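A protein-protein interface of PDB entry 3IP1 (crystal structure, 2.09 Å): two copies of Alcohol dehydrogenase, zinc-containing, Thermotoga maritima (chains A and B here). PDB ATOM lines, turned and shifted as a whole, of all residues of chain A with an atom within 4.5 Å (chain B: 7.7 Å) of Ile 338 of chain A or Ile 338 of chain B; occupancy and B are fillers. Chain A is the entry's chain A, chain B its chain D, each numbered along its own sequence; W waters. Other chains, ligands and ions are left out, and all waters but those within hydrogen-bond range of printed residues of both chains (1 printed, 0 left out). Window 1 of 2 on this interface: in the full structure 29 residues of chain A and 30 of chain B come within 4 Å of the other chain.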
ATOM      1  N   TRP A 297      23.315  -8.619  26.822  1.00  0.00           N
ATOM      2  CA  TRP A 297      24.021  -7.407  27.208  1.00  0.00           C
ATOM      3  C   TRP A 297      25.287  -7.663  28.026  1.00  0.00           C
ATOM      4  O   TRP A 297      26.321  -7.057  27.743  1.00  0.00           O
ATOM      5  CB  TRP A 297      23.111  -6.436  27.965  1.00  0.00           C
ATOM      6  CG  TRP A 297      23.566  -5.035  27.831  1.00  0.00           C
ATOM      7  CD1 TRP A 297      24.310  -4.327  28.723  1.00  0.00           C
ATOM      8  CD2 TRP A 297      23.332  -4.159  26.714  1.00  0.00           C
ATOM      9  NE1 TRP A 297      24.547  -3.060  28.242  1.00  0.00           N
ATOM     10  CE2 TRP A 297      23.963  -2.934  27.006  1.00  0.00           C
ATOM     11  CE3 TRP A 297      22.645  -4.295  25.501  1.00  0.00           C
ATOM     12  CZ2 TRP A 297      23.921  -1.835  26.128  1.00  0.00           C
ATOM     13  CZ3 TRP A 297      22.606  -3.210  24.619  1.00  0.00           C
ATOM     14  CH2 TRP A 297      23.240  -1.996  24.942  1.00  0.00           C
ATOM     15  N   VAL A 314      27.074   0.368  20.372  1.00  0.00           N
ATOM     16  CA  VAL A 314      26.063  -0.679  20.362  1.00  0.00           C
ATOM     17  C   VAL A 314      24.783  -0.086  19.806  1.00  0.00           C
ATOM     18  O   VAL A 314      24.224   0.844  20.370  1.00  0.00           O
ATOM     19  CB  VAL A 314      25.781  -1.302  21.727  1.00  0.00           C
ATOM     20  CG1 VAL A 314      24.874  -2.539  21.552  1.00  0.00           C
ATOM     21  CG2 VAL A 314      27.047  -1.695  22.403  1.00  0.00           C
ATOM     22  N   ILE A 316      20.909  -0.682  18.933  1.00  0.00           N
ATOM     23  CA  ILE A 316      19.776  -1.540  19.307  1.00  0.00           C
ATOM     24  C   ILE A 316      18.645  -1.387  18.299  1.00  0.00           C
ATOM     25  O   ILE A 316      18.062  -0.318  18.178  1.00  0.00           O
ATOM     26  CB  ILE A 316      19.266  -1.229  20.736  1.00  0.00           C
ATOM     27  CG1 ILE A 316      20.386  -1.449  21.760  1.00  0.00           C
ATOM     28  CG2 ILE A 316      18.063  -2.145  21.099  1.00  0.00           C
ATOM     29  CD1 ILE A 316      20.214  -0.654  23.072  1.00  0.00           C
ATOM     30  N   LEU A 326      22.483  -2.232  32.085  1.00  0.00           N
ATOM     31  CA  LEU A 326      23.570  -1.357  31.669  1.00  0.00           C
ATOM     32  C   LEU A 326      24.542  -1.027  32.803  1.00  0.00           C
ATOM     33  O   LEU A 326      24.159  -0.529  33.847  1.00  0.00           O
ATOM     34  CB  LEU A 326      22.985  -0.053  31.092  1.00  0.00           C
ATOM     35  CG  LEU A 326      23.950   1.091  30.775  1.00  0.00           C
ATOM     36  CD1 LEU A 326      24.971   0.641  29.732  1.00  0.00           C
ATOM     37  CD2 LEU A 326      23.174   2.334  30.292  1.00  0.00           C
ATOM     38  N   PHE A 331      30.955   1.736  29.466  1.00  0.00           N
ATOM     39  CA  PHE A 331      30.863   2.776  28.442  1.00  0.00           C
ATOM     40  C   PHE A 331      31.769   3.975  28.693  1.00  0.00           C
ATOM     41  O   PHE A 331      32.390   4.459  27.751  1.00  0.00           O
ATOM     42  CB  PHE A 331      29.391   3.135  28.117  1.00  0.00           C
ATOM     43  CG  PHE A 331      28.667   1.981  27.507  1.00  0.00           C
ATOM     44  CD1 PHE A 331      28.561   1.865  26.122  1.00  0.00           C
ATOM     45  CD2 PHE A 331      28.218   0.922  28.310  1.00  0.00           C
ATOM     46  CE1 PHE A 331      27.976   0.729  25.538  1.00  0.00           C
ATOM     47  CE2 PHE A 331      27.637  -0.210  27.733  1.00  0.00           C
ATOM     48  CZ  PHE A 331      27.519  -0.309  26.344  1.00  0.00           C
ATOM     49  N   GLN A 337      29.544   3.841  23.161  1.00  0.00           N
ATOM     50  CA  GLN A 337      28.218   4.455  23.154  1.00  0.00           C
ATOM     51  C   GLN A 337      27.111   3.486  22.701  1.00  0.00           C
ATOM     52  O   GLN A 337      27.373   2.421  22.159  1.00  0.00           O
ATOM     53  CB  GLN A 337      28.184   5.750  22.312  1.00  0.00           C
ATOM     54  CG  GLN A 337      28.773   5.652  20.887  1.00  0.00           C
ATOM     55  CD  GLN A 337      30.335   5.731  20.833  1.00  0.00           C
ATOM     56  OE1 GLN A 337      31.003   6.375  21.667  1.00  0.00           O
ATOM     57  NE2 GLN A 337      30.902   5.065  19.849  1.00  0.00           N
ATOM     58  N   ILE A 338      25.875   3.908  22.939  1.00  0.00           N
ATOM     59  CA  ILE A 338      24.686   3.121  22.686  1.00  0.00           C
ATOM     60  C   ILE A 338      23.705   4.006  21.939  1.00  0.00           C
ATOM     61  O   ILE A 338      23.346   5.076  22.423  1.00  0.00           O
ATOM     62  CB  ILE A 338      23.991   2.712  24.023  1.00  0.00           C
ATOM     63  CG1 ILE A 338      24.959   1.944  24.943  1.00  0.00           C
ATOM     64  CG2 ILE A 338      22.707   1.895  23.742  1.00  0.00           C
ATOM     65  CD1 ILE A 338      24.453   1.840  26.356  1.00  0.00           C
ATOM     66  N   VAL A 339      23.276   3.544  20.772  1.00  0.00           N
ATOM     67  CA  VAL A 339      22.264   4.237  19.979  1.00  0.00           C
ATOM     68  C   VAL A 339      21.067   3.310  19.749  1.00  0.00           C
ATOM     69  O   VAL A 339      21.211   2.101  19.536  1.00  0.00           O
ATOM     70  CB  VAL A 339      22.818   4.770  18.598  1.00  0.00           C
ATOM     71  CG1 VAL A 339      24.019   5.705  18.801  1.00  0.00           C
ATOM     72  CG2 VAL A 339      23.219   3.629  17.673  1.00  0.00           C
ATOM     73  N   GLY A 340      19.876   3.874  19.807  1.00  0.00           N
ATOM     74  CA  GLY A 340      18.711   3.145  19.389  1.00  0.00           C
ATOM     75  C   GLY A 340      18.421   3.485  17.941  1.00  0.00           C
ATOM     76  O   GLY A 340      18.784   4.561  17.455  1.00  0.00           O
ATOM     77  N   ARG B 207      32.408  14.375  24.112  1.00  0.00           N
ATOM     78  CA  ARG B 207      31.695  13.101  24.131  1.00  0.00           C
ATOM     79  C   ARG B 207      30.207  13.294  23.798  1.00  0.00           C
ATOM     80  O   ARG B 207      29.685  12.644  22.905  1.00  0.00           O
ATOM     81  CB  ARG B 207      31.883  12.398  25.498  1.00  0.00           C
ATOM     82  CG  ARG B 207      33.298  11.794  25.716  1.00  0.00           C
ATOM     83  CD  ARG B 207      33.606  10.720  24.631  1.00  0.00           C
ATOM     84  NE  ARG B 207      32.762   9.529  24.763  1.00  0.00           N
ATOM     85  CZ  ARG B 207      32.350   8.750  23.767  1.00  0.00           C
ATOM     86  NH1 ARG B 207      32.651   9.019  22.496  1.00  0.00           N
ATOM     87  NH2 ARG B 207      31.614   7.686  24.043  1.00  0.00           N
ATOM     88  N   TRP B 297      17.626   7.651  36.324  1.00  0.00           N
ATOM     89  CA  TRP B 297      17.482   7.158  34.955  1.00  0.00           C
ATOM     90  C   TRP B 297      16.013   7.095  34.482  1.00  0.00           C
ATOM     91  O   TRP B 297      15.723   7.505  33.359  1.00  0.00           O
ATOM     92  CB  TRP B 297      18.181   5.811  34.741  1.00  0.00           C
ATOM     93  CG  TRP B 297      18.436   5.587  33.290  1.00  0.00           C
ATOM     94  CD1 TRP B 297      17.652   4.893  32.411  1.00  0.00           C
ATOM     95  CD2 TRP B 297      19.514   6.126  32.524  1.00  0.00           C
ATOM     96  NE1 TRP B 297      18.200   4.941  31.151  1.00  0.00           N
ATOM     97  CE2 TRP B 297      19.346   5.684  31.195  1.00  0.00           C
ATOM     98  CE3 TRP B 297      20.628   6.912  32.841  1.00  0.00           C
ATOM     99  CZ2 TRP B 297      20.253   6.016  30.169  1.00  0.00           C
ATOM    100  CZ3 TRP B 297      21.521   7.248  31.823  1.00  0.00           C
ATOM    101  CH2 TRP B 297      21.328   6.791  30.505  1.00  0.00           C
ATOM    102  N   GLU B 301      14.551   9.061  31.223  1.00  0.00           N
ATOM    103  CA  GLU B 301      13.877   8.318  30.174  1.00  0.00           C
ATOM    104  C   GLU B 301      12.453   8.834  29.945  1.00  0.00           C
ATOM    105  O   GLU B 301      12.013   8.984  28.793  1.00  0.00           O
ATOM    106  CB  GLU B 301      13.883   6.817  30.488  1.00  0.00           C
ATOM    107  CG  GLU B 301      15.189   6.097  30.140  1.00  0.00           C
ATOM    108  CD  GLU B 301      15.073   4.571  30.208  1.00  0.00           C
ATOM    109  OE1 GLU B 301      14.082   4.073  30.790  1.00  0.00           O
ATOM    110  OE2 GLU B 301      15.970   3.847  29.692  1.00  0.00           O
ATOM    111  N   ILE B 304      12.605  12.032  28.053  1.00  0.00           N
ATOM    112  CA  ILE B 304      12.993  11.823  26.662  1.00  0.00           C
ATOM    113  C   ILE B 304      11.786  11.262  25.887  1.00  0.00           C
ATOM    114  O   ILE B 304      11.488  11.707  24.778  1.00  0.00           O
ATOM    115  CB  ILE B 304      14.238  10.898  26.543  1.00  0.00           C
ATOM    116  CG1 ILE B 304      15.503  11.622  27.033  1.00  0.00           C
ATOM    117  CG2 ILE B 304      14.459  10.456  25.102  1.00  0.00           C
ATOM    118  CD1 ILE B 304      16.721  10.700  27.220  1.00  0.00           C
ATOM    119  N   ALA B 312      18.107  13.309  21.424  1.00  0.00           N
ATOM    120  CA  ALA B 312      18.671  13.631  22.724  1.00  0.00           C
ATOM    121  C   ALA B 312      19.872  12.735  22.989  1.00  0.00           C
ATOM    122  O   ALA B 312      19.904  11.561  22.602  1.00  0.00           O
ATOM    123  CB  ALA B 312      17.631  13.485  23.834  1.00  0.00           C
ATOM    124  N   THR B 313      20.878  13.317  23.619  1.00  0.00           N
ATOM    125  CA  THR B 313      21.999  12.528  24.096  1.00  0.00           C
ATOM    126  C   THR B 313      22.046  12.571  25.613  1.00  0.00           C
ATOM    127  O   THR B 313      21.907  13.649  26.210  1.00  0.00           O
ATOM    128  CB  THR B 313      23.344  13.042  23.498  1.00  0.00           C
ATOM    129  OG1 THR B 313      23.269  12.966  22.070  1.00  0.00           O
ATOM    130  CG2 THR B 313      24.515  12.170  23.966  1.00  0.00           C
ATOM    131  N   VAL B 314      22.255  11.405  26.229  1.00  0.00           N
ATOM    132  CA  VAL B 314      22.555  11.343  27.659  1.00  0.00           C
ATOM    133  C   VAL B 314      24.056  11.052  27.861  1.00  0.00           C
ATOM    134  O   VAL B 314      24.575  10.004  27.431  1.00  0.00           O
ATOM    135  CB  VAL B 314      21.696  10.280  28.398  1.00  0.00           C
ATOM    136  CG1 VAL B 314      22.023  10.276  29.910  1.00  0.00           C
ATOM    137  CG2 VAL B 314      20.192  10.524  28.146  1.00  0.00           C
ATOM    138  N   ALA B 315      24.738  12.011  28.484  1.00  0.00           N
ATOM    139  CA  ALA B 315      26.156  11.879  28.817  1.00  0.00           C
ATOM    140  C   ALA B 315      26.346  11.437  30.264  1.00  0.00           C
ATOM    141  O   ALA B 315      25.915  12.119  31.197  1.00  0.00           O
ATOM    142  CB  ALA B 315      26.902  13.208  28.554  1.00  0.00           C
ATOM    143  N   ILE B 316      27.009  10.299  30.454  1.00  0.00           N
ATOM    144  CA  ILE B 316      27.229   9.785  31.812  1.00  0.00           C
ATOM    145  C   ILE B 316      28.671  10.057  32.261  1.00  0.00           C
ATOM    146  O   ILE B 316      29.624   9.424  31.751  1.00  0.00           O
ATOM    147  CB  ILE B 316      26.933   8.279  31.917  1.00  0.00           C
ATOM    148  CG1 ILE B 316      25.519   7.961  31.418  1.00  0.00           C
ATOM    149  CG2 ILE B 316      27.092   7.813  33.361  1.00  0.00           C
ATOM    150  CD1 ILE B 316      25.249   6.431  31.248  1.00  0.00           C
ATOM    151  N   ILE B 324      22.171   0.469  35.673  1.00  0.00           N
ATOM    152  CA  ILE B 324      21.204   1.411  35.165  1.00  0.00           C
ATOM    153  C   ILE B 324      20.048   0.621  34.544  1.00  0.00           C
ATOM    154  O   ILE B 324      20.273  -0.294  33.730  1.00  0.00           O
ATOM    155  CB  ILE B 324      21.840   2.305  34.089  1.00  0.00           C
ATOM    156  CG1 ILE B 324      22.828   3.283  34.719  1.00  0.00           C
ATOM    157  CG2 ILE B 324      20.755   3.034  33.267  1.00  0.00           C
ATOM    158  CD1 ILE B 324      23.814   3.850  33.730  1.00  0.00           C
ATOM    159  N   LEU B 326      18.034   0.357  31.934  1.00  0.00           N
ATOM    160  CA  LEU B 326      17.869   0.898  30.578  1.00  0.00           C
ATOM    161  C   LEU B 326      16.702   0.292  29.805  1.00  0.00           C
ATOM    162  O   LEU B 326      16.593  -0.925  29.670  1.00  0.00           O
ATOM    163  CB  LEU B 326      19.168   0.778  29.777  1.00  0.00           C
ATOM    164  CG  LEU B 326      19.111   1.030  28.263  1.00  0.00           C
ATOM    165  CD1 LEU B 326      18.823   2.500  27.940  1.00  0.00           C
ATOM    166  CD2 LEU B 326      20.411   0.576  27.641  1.00  0.00           C
ATOM    167  N   THR B 327      15.852   1.164  29.276  1.00  0.00           N
ATOM    168  CA  THR B 327      14.769   0.757  28.399  1.00  0.00           C
ATOM    169  C   THR B 327      15.147   1.106  26.963  1.00  0.00           C
ATOM    170  O   THR B 327      15.096   2.281  26.556  1.00  0.00           O
ATOM    171  CB  THR B 327      13.448   1.472  28.775  1.00  0.00           C
ATOM    172  OG1 THR B 327      13.319   1.522  30.198  1.00  0.00           O
ATOM    173  CG2 THR B 327      12.225   0.757  28.158  1.00  0.00           C
ATOM    174  N   GLY B 328      15.533   0.081  26.205  1.00  0.00           N
ATOM    175  CA  GLY B 328      15.956   0.236  24.812  1.00  0.00           C
ATOM    176  C   GLY B 328      14.964   1.009  23.949  1.00  0.00           C
ATOM    177  O   GLY B 328      15.346   1.891  23.174  1.00  0.00           O
ATOM    178  N   PHE B 331      15.026   4.842  23.604  1.00  0.00           N
ATOM    179  CA  PHE B 331      16.088   5.376  22.765  1.00  0.00           C
ATOM    180  C   PHE B 331      15.854   5.140  21.283  1.00  0.00           C
ATOM    181  O   PHE B 331      16.175   6.004  20.468  1.00  0.00           O
ATOM    182  CB  PHE B 331      17.434   4.885  23.268  1.00  0.00           C
ATOM    183  CG  PHE B 331      17.786   5.481  24.603  1.00  0.00           C
ATOM    184  CD1 PHE B 331      18.554   6.639  24.677  1.00  0.00           C
ATOM    185  CD2 PHE B 331      17.274   4.931  25.784  1.00  0.00           C
ATOM    186  CE1 PHE B 331      18.846   7.226  25.910  1.00  0.00           C
ATOM    187  CE2 PHE B 331      17.555   5.507  27.027  1.00  0.00           C
ATOM    188  CZ  PHE B 331      18.353   6.645  27.095  1.00  0.00           C
ATOM    189  N   ALA B 336      17.484   8.598  20.263  1.00  0.00           N
ATOM    190  CA  ALA B 336      18.320   9.148  21.303  1.00  0.00           C
ATOM    191  C   ALA B 336      19.509   8.238  21.545  1.00  0.00           C
ATOM    192  O   ALA B 336      19.532   7.101  21.086  1.00  0.00           O
ATOM    193  CB  ALA B 336      17.504   9.359  22.578  1.00  0.00           C
ATOM    194  N   GLN B 337      20.507   8.742  22.254  1.00  0.00           N
ATOM    195  CA  GLN B 337      21.706   7.944  22.483  1.00  0.00           C
ATOM    196  C   GLN B 337      22.324   8.216  23.846  1.00  0.00           C
ATOM    197  O   GLN B 337      21.989   9.206  24.486  1.00  0.00           O
ATOM    198  CB  GLN B 337      22.739   8.134  21.348  1.00  0.00           C
ATOM    199  CG  GLN B 337      23.077   9.563  20.953  1.00  0.00           C
ATOM    200  CD  GLN B 337      22.039  10.196  20.014  1.00  0.00           C
ATOM    201  OE1 GLN B 337      21.445   9.525  19.159  1.00  0.00           O
ATOM    202  NE2 GLN B 337      21.809  11.494  20.181  1.00  0.00           N
ATOM    203  N   ILE B 338      23.247   7.338  24.239  1.00  0.00           N
ATOM    204  CA  ILE B 338      23.918   7.370  25.528  1.00  0.00           C
ATOM    205  C   ILE B 338      25.413   7.299  25.271  1.00  0.00           C
ATOM    206  O   ILE B 338      25.881   6.399  24.588  1.00  0.00           O
ATOM    207  CB  ILE B 338      23.520   6.127  26.386  1.00  0.00           C
ATOM    208  CG1 ILE B 338      22.001   6.062  26.553  1.00  0.00           C
ATOM    209  CG2 ILE B 338      24.267   6.147  27.751  1.00  0.00           C
ATOM    210  CD1 ILE B 338      21.414   4.657  26.918  1.00  0.00           C
ATOM    211  N   VAL B 339      26.154   8.251  25.820  1.00  0.00           N
ATOM    212  CA  VAL B 339      27.597   8.260  25.718  1.00  0.00           C
ATOM    213  C   VAL B 339      28.193   8.269  27.123  1.00  0.00           C
ATOM    214  O   VAL B 339      27.652   8.879  28.043  1.00  0.00           O
ATOM    215  CB  VAL B 339      28.123   9.508  24.924  1.00  0.00           C
ATOM    216  CG1 VAL B 339      27.645   9.472  23.435  1.00  0.00           C
ATOM    217  CG2 VAL B 339      27.707  10.840  25.627  1.00  0.00           C
ATOM    218  N   GLY B 340      29.303   7.563  27.289  1.00  0.00           N
ATOM    219  CA  GLY B 340      30.085   7.672  28.522  1.00  0.00           C
ATOM    220  C   GLY B 340      31.115   8.765  28.340  1.00  0.00           C
ATOM    221  O   GLY B 340      31.459   9.127  27.203  1.00  0.00           O
HETATM  222  O   HOH W   1      32.933   7.234  20.042  1.00  0.00           O
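The backbone NH of Gly 340 of chain A lies within hydrogen-bond range of the backbone carbonyl oxygen of Ala 336 of chain B. N of Ile 338 of chain B lies within hydrogen-bond range of O of Ile 338 of chain A (2.9 Å). The backbone carbonyl oxygen (O) of Leu 326 of chain A lies within hydrogen-bond range of the backbone NH (N) of Ile 324 of chain B, 2.9 Å away. The side-chain amide oxygen (OE1) of Gln 337 of chain A is in hydrogen-bond range of the guanidinium group (NH2) of Arg 207 of chain B (2.8 Å).
The backbone carbonyl oxygen (O) of Ala 312 of chain B is in hydrogen-bond range of the backbone NH (N) of Gln 337 of chain B, 2.9 Å away. The side-chain hydroxyl (OG1) of Thr 313 of chain B sits at hydrogen-bond distance from the side-chain amide nitrogen (NE2) of Gln 337 of chain B (2.8 Å). N of Val 314 of chain A sits at hydrogen-bond distance from O of Gln 337 of chain A (2.7 Å). The backbone NH (N) of Val 314 of chain B lies within hydrogen-bond range of the backbone carbonyl oxygen (O) of Gln 337 of chain B, 2.8 Å away. The backbone NH of Ile 316 of chain B is in hydrogen-bond range of the backbone carbonyl oxygen of Val 339 of chain B. NE of Arg 207 of chain B sits at hydrogen-bond distance from O of Gly 340 of chain B (2.8 Å).
Among the printed residues, pairs that only touch across the chains: Gln 337 of chain A with Ile 338 of chain B (3.3 Å), Gln 337 of chain A with Val 339 of chain B (3.9 Å), Ile 338 of chain A with Gln 337 of chain B (3.3 Å), Val 339 of chain A with Gln 337 of chain B (3.7 Å) and Gly 340 of chain A with Phe 331 of chain B (3.97 Å).
Phe 331 of chain A touches none of the printed residues of chain B. Of the printed residues of chain B, Gln 337 of chain A touches Arg 207, Ile 338 and Val 339. Ile 338 of chain A touches just these residues of chain B: Gln 337 and Ile 338. Printed residues of chain A within 4 Å of Phe 331 of chain B: Gly 340 (3.97 Å). Of the printed residues of chain A, Ala 336 of chain B touches Gly 340. Of the printed residues of chain A, Gln 337 of chain B touches Ile 338 (3.3 Å) and Val 339 (3.7 Å). Ile 338 of chain B touches just these residues of chain A: Gln 337 and Ile 338. The nearest residue of chain B that does not touch Ile 338 of chain A is Leu 326 of chain B (4.4 Å). The nearest printed residue of chain B that does not touch Gly 340 of chain A is Gln 337 of chain B (5.2 Å).
Along chain A the printed residues that touch a printed residue of chain B span positions 326 to 340. Of the 19 printed residues of chain B, 7 touch a printed residue of chain A. Hydrophobic or aromatic side chains of chain B within 4 Å of the printed part of chain A: Ile 324 and Val 339. Among the printed residues, no Asp or Glu carboxylate lies within 4 Å of a Lys or Arg side-chain nitrogen of the other chain.
Gln 337 of chain A touches Ile 338 of chain B, and with the chains exchanged Ile 338 of chain A touches Gln 337 of chain B. Gln 337 of chain A touches Val 339 of chain B, and with the chains exchanged Val 339 of chain A touches Gln 337 of chain B. Ile 338 of chain A touches its own counterpart, Ile 338 of chain B. Gly 340 of chain A touches Phe 331 of chain B, but with the chains exchanged Phe 331 of chain A does not touch Gly 340 of chain B (4.03 Å). Of the 9 pairs that touch across the chains among the printed residues, 5 have their exchanged pair printed and touching as well.
Water W1 lies within hydrogen-bond range of OE1 of Gln 337 of chain A (2.7 Å) and NH1 of Arg 207 of chain B (3.0 Å).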
